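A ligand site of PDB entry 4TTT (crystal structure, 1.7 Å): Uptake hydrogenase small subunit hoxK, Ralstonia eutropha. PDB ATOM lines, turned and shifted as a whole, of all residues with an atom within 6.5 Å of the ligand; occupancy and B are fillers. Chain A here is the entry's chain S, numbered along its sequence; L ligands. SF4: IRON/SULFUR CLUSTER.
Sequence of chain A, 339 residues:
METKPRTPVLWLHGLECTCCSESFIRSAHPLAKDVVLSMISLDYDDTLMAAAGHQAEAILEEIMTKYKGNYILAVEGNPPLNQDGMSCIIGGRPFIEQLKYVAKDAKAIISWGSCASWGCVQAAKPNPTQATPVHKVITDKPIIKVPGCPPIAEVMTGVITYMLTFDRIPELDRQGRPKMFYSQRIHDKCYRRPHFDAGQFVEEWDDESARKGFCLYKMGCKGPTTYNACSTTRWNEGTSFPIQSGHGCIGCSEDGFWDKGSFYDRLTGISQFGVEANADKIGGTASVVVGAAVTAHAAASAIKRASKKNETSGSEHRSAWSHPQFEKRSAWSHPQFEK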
ATOM      1  N   ILE A 186     -23.516  20.679  -0.312  1.00  0.00           N
ATOM      2  CA  ILE A 186     -22.283  20.710  -1.115  1.00  0.00           C
ATOM      3  C   ILE A 186     -21.219  19.775  -0.538  1.00  0.00           C
ATOM      4  O   ILE A 186     -20.563  19.026  -1.275  1.00  0.00           O
ATOM      5  CB  ILE A 186     -21.660  22.141  -1.173  1.00  0.00           C
ATOM      6  CG1 ILE A 186     -22.654  23.198  -1.672  1.00  0.00           C
ATOM      7  CG2 ILE A 186     -20.403  22.169  -2.034  1.00  0.00           C
ATOM      8  CD1 ILE A 186     -23.329  22.869  -2.976  1.00  0.00           C
ATOM      9  N   HIS A 187     -21.070  19.836   0.785  1.00  0.00           N
ATOM     10  CA  HIS A 187     -20.067  19.080   1.560  1.00  0.00           C
ATOM     11  C   HIS A 187     -20.224  17.552   1.499  1.00  0.00           C
ATOM     12  O   HIS A 187     -19.263  16.823   1.788  1.00  0.00           O
ATOM     13  CB  HIS A 187     -20.152  19.570   3.013  1.00  0.00           C
ATOM     14  CG  HIS A 187     -19.095  19.024   3.922  1.00  0.00           C
ATOM     15  ND1 HIS A 187     -17.819  19.546   3.964  1.00  0.00           N
ATOM     16  CD2 HIS A 187     -19.131  18.053   4.870  1.00  0.00           C
ATOM     17  CE1 HIS A 187     -17.111  18.899   4.877  1.00  0.00           C
ATOM     18  NE2 HIS A 187     -17.879  17.994   5.433  1.00  0.00           N
ATOM     19  N   ASP A 188     -21.403  17.066   1.128  1.00  0.00           N
ATOM     20  CA  ASP A 188     -21.650  15.612   1.089  1.00  0.00           C
ATOM     21  C   ASP A 188     -20.759  14.899   0.056  1.00  0.00           C
ATOM     22  O   ASP A 188     -20.133  13.905   0.387  1.00  0.00           O
ATOM     23  CB  ASP A 188     -23.130  15.313   0.812  1.00  0.00           C
ATOM     24  CG  ASP A 188     -24.048  15.689   1.972  1.00  0.00           C
ATOM     25  OD1 ASP A 188     -23.567  15.870   3.116  1.00  0.00           O
ATOM     26  OD2 ASP A 188     -25.273  15.813   1.747  1.00  0.00           O
ATOM     27  N   CYS A 190     -18.519  16.753  -2.163  1.00  0.00           N
ATOM     28  CA  CYS A 190     -17.413  17.605  -2.577  1.00  0.00           C
ATOM     29  C   CYS A 190     -16.124  16.788  -2.685  1.00  0.00           C
ATOM     30  O   CYS A 190     -15.779  16.042  -1.770  1.00  0.00           O
ATOM     31  CB  CYS A 190     -17.208  18.735  -1.571  1.00  0.00           C
ATOM     32  SG  CYS A 190     -15.760  19.768  -1.941  1.00  0.00           S
ATOM     33  N   TYR A 191     -15.423  16.931  -3.807  1.00  0.00           N
ATOM     34  CA  TYR A 191     -14.231  16.135  -4.095  1.00  0.00           C
ATOM     35  C   TYR A 191     -13.070  16.411  -3.121  1.00  0.00           C
ATOM     36  O   TYR A 191     -12.154  15.598  -3.030  1.00  0.00           O
ATOM     37  CB  TYR A 191     -13.772  16.312  -5.544  1.00  0.00           C
ATOM     38  CG  TYR A 191     -12.950  17.564  -5.765  1.00  0.00           C
ATOM     39  CD1 TYR A 191     -13.561  18.810  -5.837  1.00  0.00           C
ATOM     40  CD2 TYR A 191     -11.556  17.497  -5.858  1.00  0.00           C
ATOM     41  CE1 TYR A 191     -12.806  19.963  -6.017  1.00  0.00           C
ATOM     42  CE2 TYR A 191     -10.802  18.636  -6.037  1.00  0.00           C
ATOM     43  CZ  TYR A 191     -11.429  19.869  -6.111  1.00  0.00           C
ATOM     44  OH  TYR A 191     -10.691  21.009  -6.283  1.00  0.00           O
ATOM     45  N   ARG A 192     -13.106  17.540  -2.421  1.00  0.00           N
ATOM     46  CA  ARG A 192     -12.118  17.855  -1.387  1.00  0.00           C
ATOM     47  C   ARG A 192     -12.453  17.231  -0.025  1.00  0.00           C
ATOM     48  O   ARG A 192     -11.699  17.419   0.922  1.00  0.00           O
ATOM     49  CB  ARG A 192     -11.956  19.362  -1.243  1.00  0.00           C
ATOM     50  CG  ARG A 192     -11.514  20.061  -2.518  1.00  0.00           C
ATOM     51  CD  ARG A 192     -10.971  21.454  -2.264  1.00  0.00           C
ATOM     52  NE  ARG A 192     -10.595  22.089  -3.528  1.00  0.00           N
ATOM     53  CZ  ARG A 192      -9.698  23.065  -3.667  1.00  0.00           C
ATOM     54  NH1 ARG A 192      -9.044  23.576  -2.636  1.00  0.00           N
ATOM     55  NH2 ARG A 192      -9.446  23.542  -4.887  1.00  0.00           N
ATOM     56  N   ARG A 193     -13.563  16.517   0.080  1.00  0.00           N
ATOM     57  CA  ARG A 193     -14.002  15.924   1.352  1.00  0.00           C
ATOM     58  C   ARG A 193     -12.967  14.993   2.016  1.00  0.00           C
ATOM     59  O   ARG A 193     -12.810  15.030   3.240  1.00  0.00           O
ATOM     60  CB  ARG A 193     -15.356  15.223   1.171  1.00  0.00           C
ATOM     61  CG  ARG A 193     -15.961  14.582   2.416  1.00  0.00           C
ATOM     62  CD  ARG A 193     -16.276  15.601   3.498  1.00  0.00           C
ATOM     63  NE  ARG A 193     -16.874  14.979   4.673  1.00  0.00           N
ATOM     64  CZ  ARG A 193     -18.134  14.571   4.772  1.00  0.00           C
ATOM     65  NH1 ARG A 193     -18.988  14.719   3.758  1.00  0.00           N
ATOM     66  NH2 ARG A 193     -18.566  14.011   5.903  1.00  0.00           N
ATOM     67  N   PRO A 194     -12.246  14.159   1.232  1.00  0.00           N
ATOM     68  CA  PRO A 194     -11.184  13.374   1.865  1.00  0.00           C
ATOM     69  C   PRO A 194     -10.135  14.219   2.589  1.00  0.00           C
ATOM     70  O   PRO A 194      -9.660  13.810   3.648  1.00  0.00           O
ATOM     71  CB  PRO A 194     -10.577  12.602   0.694  1.00  0.00           C
ATOM     72  CG  PRO A 194     -11.729  12.418  -0.240  1.00  0.00           C
ATOM     73  CD  PRO A 194     -12.526  13.684  -0.142  1.00  0.00           C
ATOM     74  N   HIS A 195      -9.811  15.402   2.050  1.00  0.00           N
ATOM     75  CA  HIS A 195      -8.915  16.325   2.745  1.00  0.00           C
ATOM     76  C   HIS A 195      -9.538  16.859   4.043  1.00  0.00           C
ATOM     77  O   HIS A 195      -8.848  16.954   5.052  1.00  0.00           O
ATOM     78  CB  HIS A 195      -8.521  17.504   1.843  1.00  0.00           C
ATOM     79  CG  HIS A 195      -7.662  17.105   0.673  1.00  0.00           C
ATOM     80  ND1 HIS A 195      -6.445  16.469   0.831  1.00  0.00           N
ATOM     81  CD2 HIS A 195      -7.838  17.267  -0.661  1.00  0.00           C
ATOM     82  CE1 HIS A 195      -5.926  16.246  -0.361  1.00  0.00           C
ATOM     83  NE2 HIS A 195      -6.745  16.711  -1.278  1.00  0.00           N
ATOM     84  N   PHE A 196     -10.815  17.218   3.994  1.00  0.00           N
ATOM     85  CA  PHE A 196     -11.525  17.652   5.198  1.00  0.00           C
ATOM     86  C   PHE A 196     -11.472  16.582   6.286  1.00  0.00           C
ATOM     87  O   PHE A 196     -11.157  16.865   7.438  1.00  0.00           O
ATOM     88  CB  PHE A 196     -12.989  17.983   4.885  1.00  0.00           C
ATOM     89  CG  PHE A 196     -13.801  18.349   6.094  1.00  0.00           C
ATOM     90  CD1 PHE A 196     -13.910  19.666   6.492  1.00  0.00           C
ATOM     91  CD2 PHE A 196     -14.469  17.373   6.821  1.00  0.00           C
ATOM     92  CE1 PHE A 196     -14.663  20.025   7.610  1.00  0.00           C
ATOM     93  CE2 PHE A 196     -15.223  17.718   7.940  1.00  0.00           C
ATOM     94  CZ  PHE A 196     -15.317  19.033   8.330  1.00  0.00           C
ATOM     95  N   PHE A 201      -6.161  21.321   5.392  1.00  0.00           N
ATOM     96  CA  PHE A 201      -6.810  22.595   5.059  1.00  0.00           C
ATOM     97  C   PHE A 201      -5.868  23.631   4.448  1.00  0.00           C
ATOM     98  O   PHE A 201      -4.681  23.676   4.773  1.00  0.00           O
ATOM     99  CB  PHE A 201      -7.411  23.233   6.326  1.00  0.00           C
ATOM    100  CG  PHE A 201      -8.404  22.352   7.025  1.00  0.00           C
ATOM    101  CD1 PHE A 201      -9.671  22.142   6.488  1.00  0.00           C
ATOM    102  CD2 PHE A 201      -8.083  21.740   8.236  1.00  0.00           C
ATOM    103  CE1 PHE A 201     -10.589  21.339   7.136  1.00  0.00           C
ATOM    104  CE2 PHE A 201      -9.004  20.937   8.893  1.00  0.00           C
ATOM    105  CZ  PHE A 201     -10.261  20.733   8.348  1.00  0.00           C
ATOM    106  N   PHE A 214      -6.325  21.285  -1.051  1.00  0.00           N
ATOM    107  CA  PHE A 214      -6.822  20.968   0.294  1.00  0.00           C
ATOM    108  C   PHE A 214      -8.160  21.657   0.570  1.00  0.00           C
ATOM    109  O   PHE A 214      -8.535  22.616  -0.102  1.00  0.00           O
ATOM    110  CB  PHE A 214      -5.769  21.341   1.358  1.00  0.00           C
ATOM    111  CG  PHE A 214      -4.647  20.331   1.521  1.00  0.00           C
ATOM    112  CD1 PHE A 214      -4.390  19.327   0.581  1.00  0.00           C
ATOM    113  CD2 PHE A 214      -3.802  20.413   2.629  1.00  0.00           C
ATOM    114  CE1 PHE A 214      -3.347  18.424   0.758  1.00  0.00           C
ATOM    115  CE2 PHE A 214      -2.758  19.510   2.806  1.00  0.00           C
ATOM    116  CZ  PHE A 214      -2.538  18.516   1.869  1.00  0.00           C
ATOM    117  N   CYS A 215      -8.881  21.138   1.558  1.00  0.00           N
ATOM    118  CA  CYS A 215     -10.194  21.655   1.925  1.00  0.00           C
ATOM    119  C   CYS A 215     -10.171  23.157   2.249  1.00  0.00           C
ATOM    120  O   CYS A 215      -9.200  23.666   2.827  1.00  0.00           O
ATOM    121  CB  CYS A 215     -10.749  20.873   3.102  1.00  0.00           C
ATOM    122  SG  CYS A 215     -12.239  21.569   3.839  1.00  0.00           S
ATOM    123  N   LEU A 216     -11.245  23.847   1.880  1.00  0.00           N
ATOM    124  CA  LEU A 216     -11.357  25.302   2.039  1.00  0.00           C
ATOM    125  C   LEU A 216     -12.179  25.741   3.265  1.00  0.00           C
ATOM    126  O   LEU A 216     -12.531  26.928   3.371  1.00  0.00           O
ATOM    127  CB  LEU A 216     -11.939  25.910   0.753  1.00  0.00           C
ATOM    128  CG  LEU A 216     -11.031  25.776  -0.467  1.00  0.00           C
ATOM    129  CD1 LEU A 216     -11.811  25.949  -1.764  1.00  0.00           C
ATOM    130  CD2 LEU A 216      -9.872  26.765  -0.409  1.00  0.00           C
ATOM    131  N   TYR A 217     -12.436  24.833   4.193  1.00  0.00           N
ATOM    132  CA  TYR A 217     -13.233  25.120   5.397  1.00  0.00           C
ATOM    133  C   TYR A 217     -12.675  26.305   6.198  1.00  0.00           C
ATOM    134  O   TYR A 217     -13.427  27.180   6.600  1.00  0.00           O
ATOM    135  CB  TYR A 217     -13.306  23.889   6.295  1.00  0.00           C
ATOM    136  CG  TYR A 217     -14.169  24.047   7.522  1.00  0.00           C
ATOM    137  CD1 TYR A 217     -15.517  23.717   7.503  1.00  0.00           C
ATOM    138  CD2 TYR A 217     -13.638  24.502   8.727  1.00  0.00           C
ATOM    139  CE1 TYR A 217     -16.310  23.824   8.631  1.00  0.00           C
ATOM    140  CE2 TYR A 217     -14.428  24.637   9.855  1.00  0.00           C
ATOM    141  CZ  TYR A 217     -15.765  24.299   9.808  1.00  0.00           C
ATOM    142  OH  TYR A 217     -16.557  24.420  10.936  1.00  0.00           O
ATOM    143  N   LYS A 218     -11.358  26.342   6.393  1.00  0.00           N
ATOM    144  CA  LYS A 218     -10.733  27.400   7.190  1.00  0.00           C
ATOM    145  C   LYS A 218     -10.618  28.715   6.428  1.00  0.00           C
ATOM    146  O   LYS A 218     -10.337  29.747   7.034  1.00  0.00           O
ATOM    147  CB  LYS A 218      -9.371  26.933   7.723  1.00  0.00           C
ATOM    148  CG  LYS A 218      -9.483  25.742   8.654  1.00  0.00           C
ATOM    149  CD  LYS A 218      -8.152  25.385   9.300  1.00  0.00           C
ATOM    150  CE  LYS A 218      -8.318  24.466  10.487  1.00  0.00           C
ATOM    151  NZ  LYS A 218      -7.012  24.026  11.061  1.00  0.00           N
ATOM    152  N   CYS A 221     -15.366  28.304   3.673  1.00  0.00           N
ATOM    153  CA  CYS A 221     -16.285  27.530   2.817  1.00  0.00           C
ATOM    154  C   CYS A 221     -17.567  27.176   3.561  1.00  0.00           C
ATOM    155  O   CYS A 221     -17.524  26.575   4.633  1.00  0.00           O
ATOM    156  CB  CYS A 221     -15.614  26.249   2.322  1.00  0.00           C
ATOM    157  SG  CYS A 221     -16.672  25.258   1.236  1.00  0.00           S
ATOM    158  N   LYS A 222     -18.706  27.542   2.978  1.00  0.00           N
ATOM    159  CA  LYS A 222     -20.011  27.273   3.573  1.00  0.00           C
ATOM    160  C   LYS A 222     -20.697  26.032   2.985  1.00  0.00           C
ATOM    161  O   LYS A 222     -21.899  25.819   3.181  1.00  0.00           O
ATOM    162  CB  LYS A 222     -20.904  28.503   3.453  1.00  0.00           C
ATOM    163  CG  LYS A 222     -20.320  29.762   4.104  1.00  0.00           C
ATOM    164  CD  LYS A 222     -19.874  29.525   5.538  1.00  0.00           C
ATOM    165  CE  LYS A 222     -19.575  30.806   6.302  1.00  0.00           C
ATOM    166  NZ  LYS A 222     -18.460  31.613   5.729  1.00  0.00           N
ATOM    167  N   GLY A 223     -19.930  25.187   2.301  1.00  0.00           N
ATOM    168  CA  GLY A 223     -20.439  23.930   1.764  1.00  0.00           C
ATOM    169  C   GLY A 223     -21.150  23.047   2.785  1.00  0.00           C
ATOM    170  O   GLY A 223     -22.161  22.417   2.448  1.00  0.00           O
ATOM    171  N   PRO A 224     -20.641  22.986   4.042  1.00  0.00           N
ATOM    172  CA  PRO A 224     -21.281  22.160   5.064  1.00  0.00           C
ATOM    173  C   PRO A 224     -22.689  22.545   5.490  1.00  0.00           C
ATOM    174  O   PRO A 224     -23.378  21.726   6.096  1.00  0.00           O
ATOM    175  CB  PRO A 224     -20.319  22.274   6.262  1.00  0.00           C
ATOM    176  CG  PRO A 224     -18.988  22.518   5.631  1.00  0.00           C
ATOM    177  CD  PRO A 224     -19.306  23.444   4.492  1.00  0.00           C
ATOM    178  N   PHE A 241     -16.793  24.025 -10.382  1.00  0.00           N
ATOM    179  CA  PHE A 241     -17.680  24.700  -9.438  1.00  0.00           C
ATOM    180  C   PHE A 241     -16.786  25.520  -8.497  1.00  0.00           C
ATOM    181  O   PHE A 241     -15.563  25.385  -8.556  1.00  0.00           O
ATOM    182  CB  PHE A 241     -18.633  23.709  -8.740  1.00  0.00           C
ATOM    183  CG  PHE A 241     -18.007  22.823  -7.691  1.00  0.00           C
ATOM    184  CD1 PHE A 241     -17.074  21.846  -8.038  1.00  0.00           C
ATOM    185  CD2 PHE A 241     -18.444  22.877  -6.367  1.00  0.00           C
ATOM    186  CE1 PHE A 241     -16.537  21.003  -7.078  1.00  0.00           C
ATOM    187  CE2 PHE A 241     -17.924  22.022  -5.399  1.00  0.00           C
ATOM    188  CZ  PHE A 241     -16.963  21.092  -5.753  1.00  0.00           C
ATOM    189  N   ILE A 243     -15.590  25.593  -5.532  1.00  0.00           N
ATOM    190  CA  ILE A 243     -14.560  24.913  -4.744  1.00  0.00           C
ATOM    191  C   ILE A 243     -13.461  24.317  -5.623  1.00  0.00           C
ATOM    192  O   ILE A 243     -12.280  24.398  -5.280  1.00  0.00           O
ATOM    193  CB  ILE A 243     -15.190  23.843  -3.836  1.00  0.00           C
ATOM    194  CG1 ILE A 243     -15.914  24.534  -2.662  1.00  0.00           C
ATOM    195  CG2 ILE A 243     -14.151  22.853  -3.311  1.00  0.00           C
ATOM    196  CD1 ILE A 243     -17.138  23.808  -2.160  1.00  0.00           C
ATOM    197  N   GLY A 248     -13.936  28.959  -1.573  1.00  0.00           N
ATOM    198  CA  GLY A 248     -14.975  28.319  -0.768  1.00  0.00           C
ATOM    199  C   GLY A 248     -16.361  28.683  -1.262  1.00  0.00           C
ATOM    200  O   GLY A 248     -16.574  29.747  -1.849  1.00  0.00           O
ATOM    201  N   CYS A 249     -17.313  27.791  -1.043  1.00  0.00           N
ATOM    202  CA  CYS A 249     -18.722  28.112  -1.225  1.00  0.00           C
ATOM    203  C   CYS A 249     -19.057  29.294  -0.314  1.00  0.00           C
ATOM    204  O   CYS A 249     -18.629  29.332   0.845  1.00  0.00           O
ATOM    205  CB  CYS A 249     -19.577  26.893  -0.878  1.00  0.00           C
ATOM    206  SG  CYS A 249     -21.363  27.140  -0.838  1.00  0.00           S
HETATM  207 FE1  SF4 L   1     -15.992  23.092   1.521  1.00  0.00          FE
HETATM  208 FE2  SF4 L   1     -14.055  21.387   2.415  1.00  0.00          FE
HETATM  209 FE3  SF4 L   1     -15.567  20.801   0.152  1.00  0.00          FE
HETATM  210 FE4  SF4 L   1     -16.618  20.675   2.665  1.00  0.00          FE
HETATM  211  S1  SF4 L   1     -14.969  19.386   1.811  1.00  0.00           S
HETATM  212  S2  SF4 L   1     -17.573  21.646   0.785  1.00  0.00           S
HETATM  213  S3  SF4 L   1     -15.663  22.507   3.687  1.00  0.00           S
HETATM  214  S4  SF4 L   1     -14.028  22.543   0.384  1.00  0.00           S
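A ring nitrogen (ND1) of His 187 is bound to an iron atom (FE4) of the ligand (2.1 Å). An iron atom (FE1) of the ligand is bound by the side-chain sulfur (SG) of Cys 221 (2.3 Å). The side-chain sulfur of Cys 215 binds an iron atom (FE2) of the ligand. SG of Cys 190 is bound to FE3 of the ligand, at 2.3 Å. The backbone NH (N) of Leu 216 lies close to a sulfur (S4) of the ligand (3.4 Å). A sulfur (S1) of the ligand sits close to the backbone NH (N) of Arg 193, at 3.6 Å.
The guanidinium group (NH1) of Arg 193 sits at hydrogen-bond distance from the backbone carbonyl oxygen (O) of His 187. N of His 187 is in hydrogen-bond range of O of Gly 223 (3.3 Å). The backbone NH (N) of Cys 221 is in hydrogen-bond range of the backbone carbonyl oxygen (O) of Leu 216 (3.2 Å). The backbone NH (N) of Gly 223 lies close to the side-chain sulfur (SG) of Cys 221 (3.4 Å). The backbone NH (N) of Cys 249 lies close to the side-chain sulfur (SG) of Cys 221. The backbone NH (N) of Tyr 217 lies close to the side-chain sulfur (SG) of Cys 215 (3.3 Å). NH2 of Arg 192 sits at hydrogen-bond distance from O of Ile 243. The guanidinium group of Arg 192 sits at hydrogen-bond distance from the backbone carbonyl oxygen of Phe 214 (2.8 Å).
Merely in contact with the ligand: Ile 243, Tyr 217, Arg 192, Gly 223, Pro 224 and Phe 196. Hydrophobic or aromatic side chains that line the ligand: His 187, Phe 196, Leu 216, Tyr 217, Pro 224 and Ile 243. Of the 24 residues printed, 12 come within 4 Å of the ligand.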
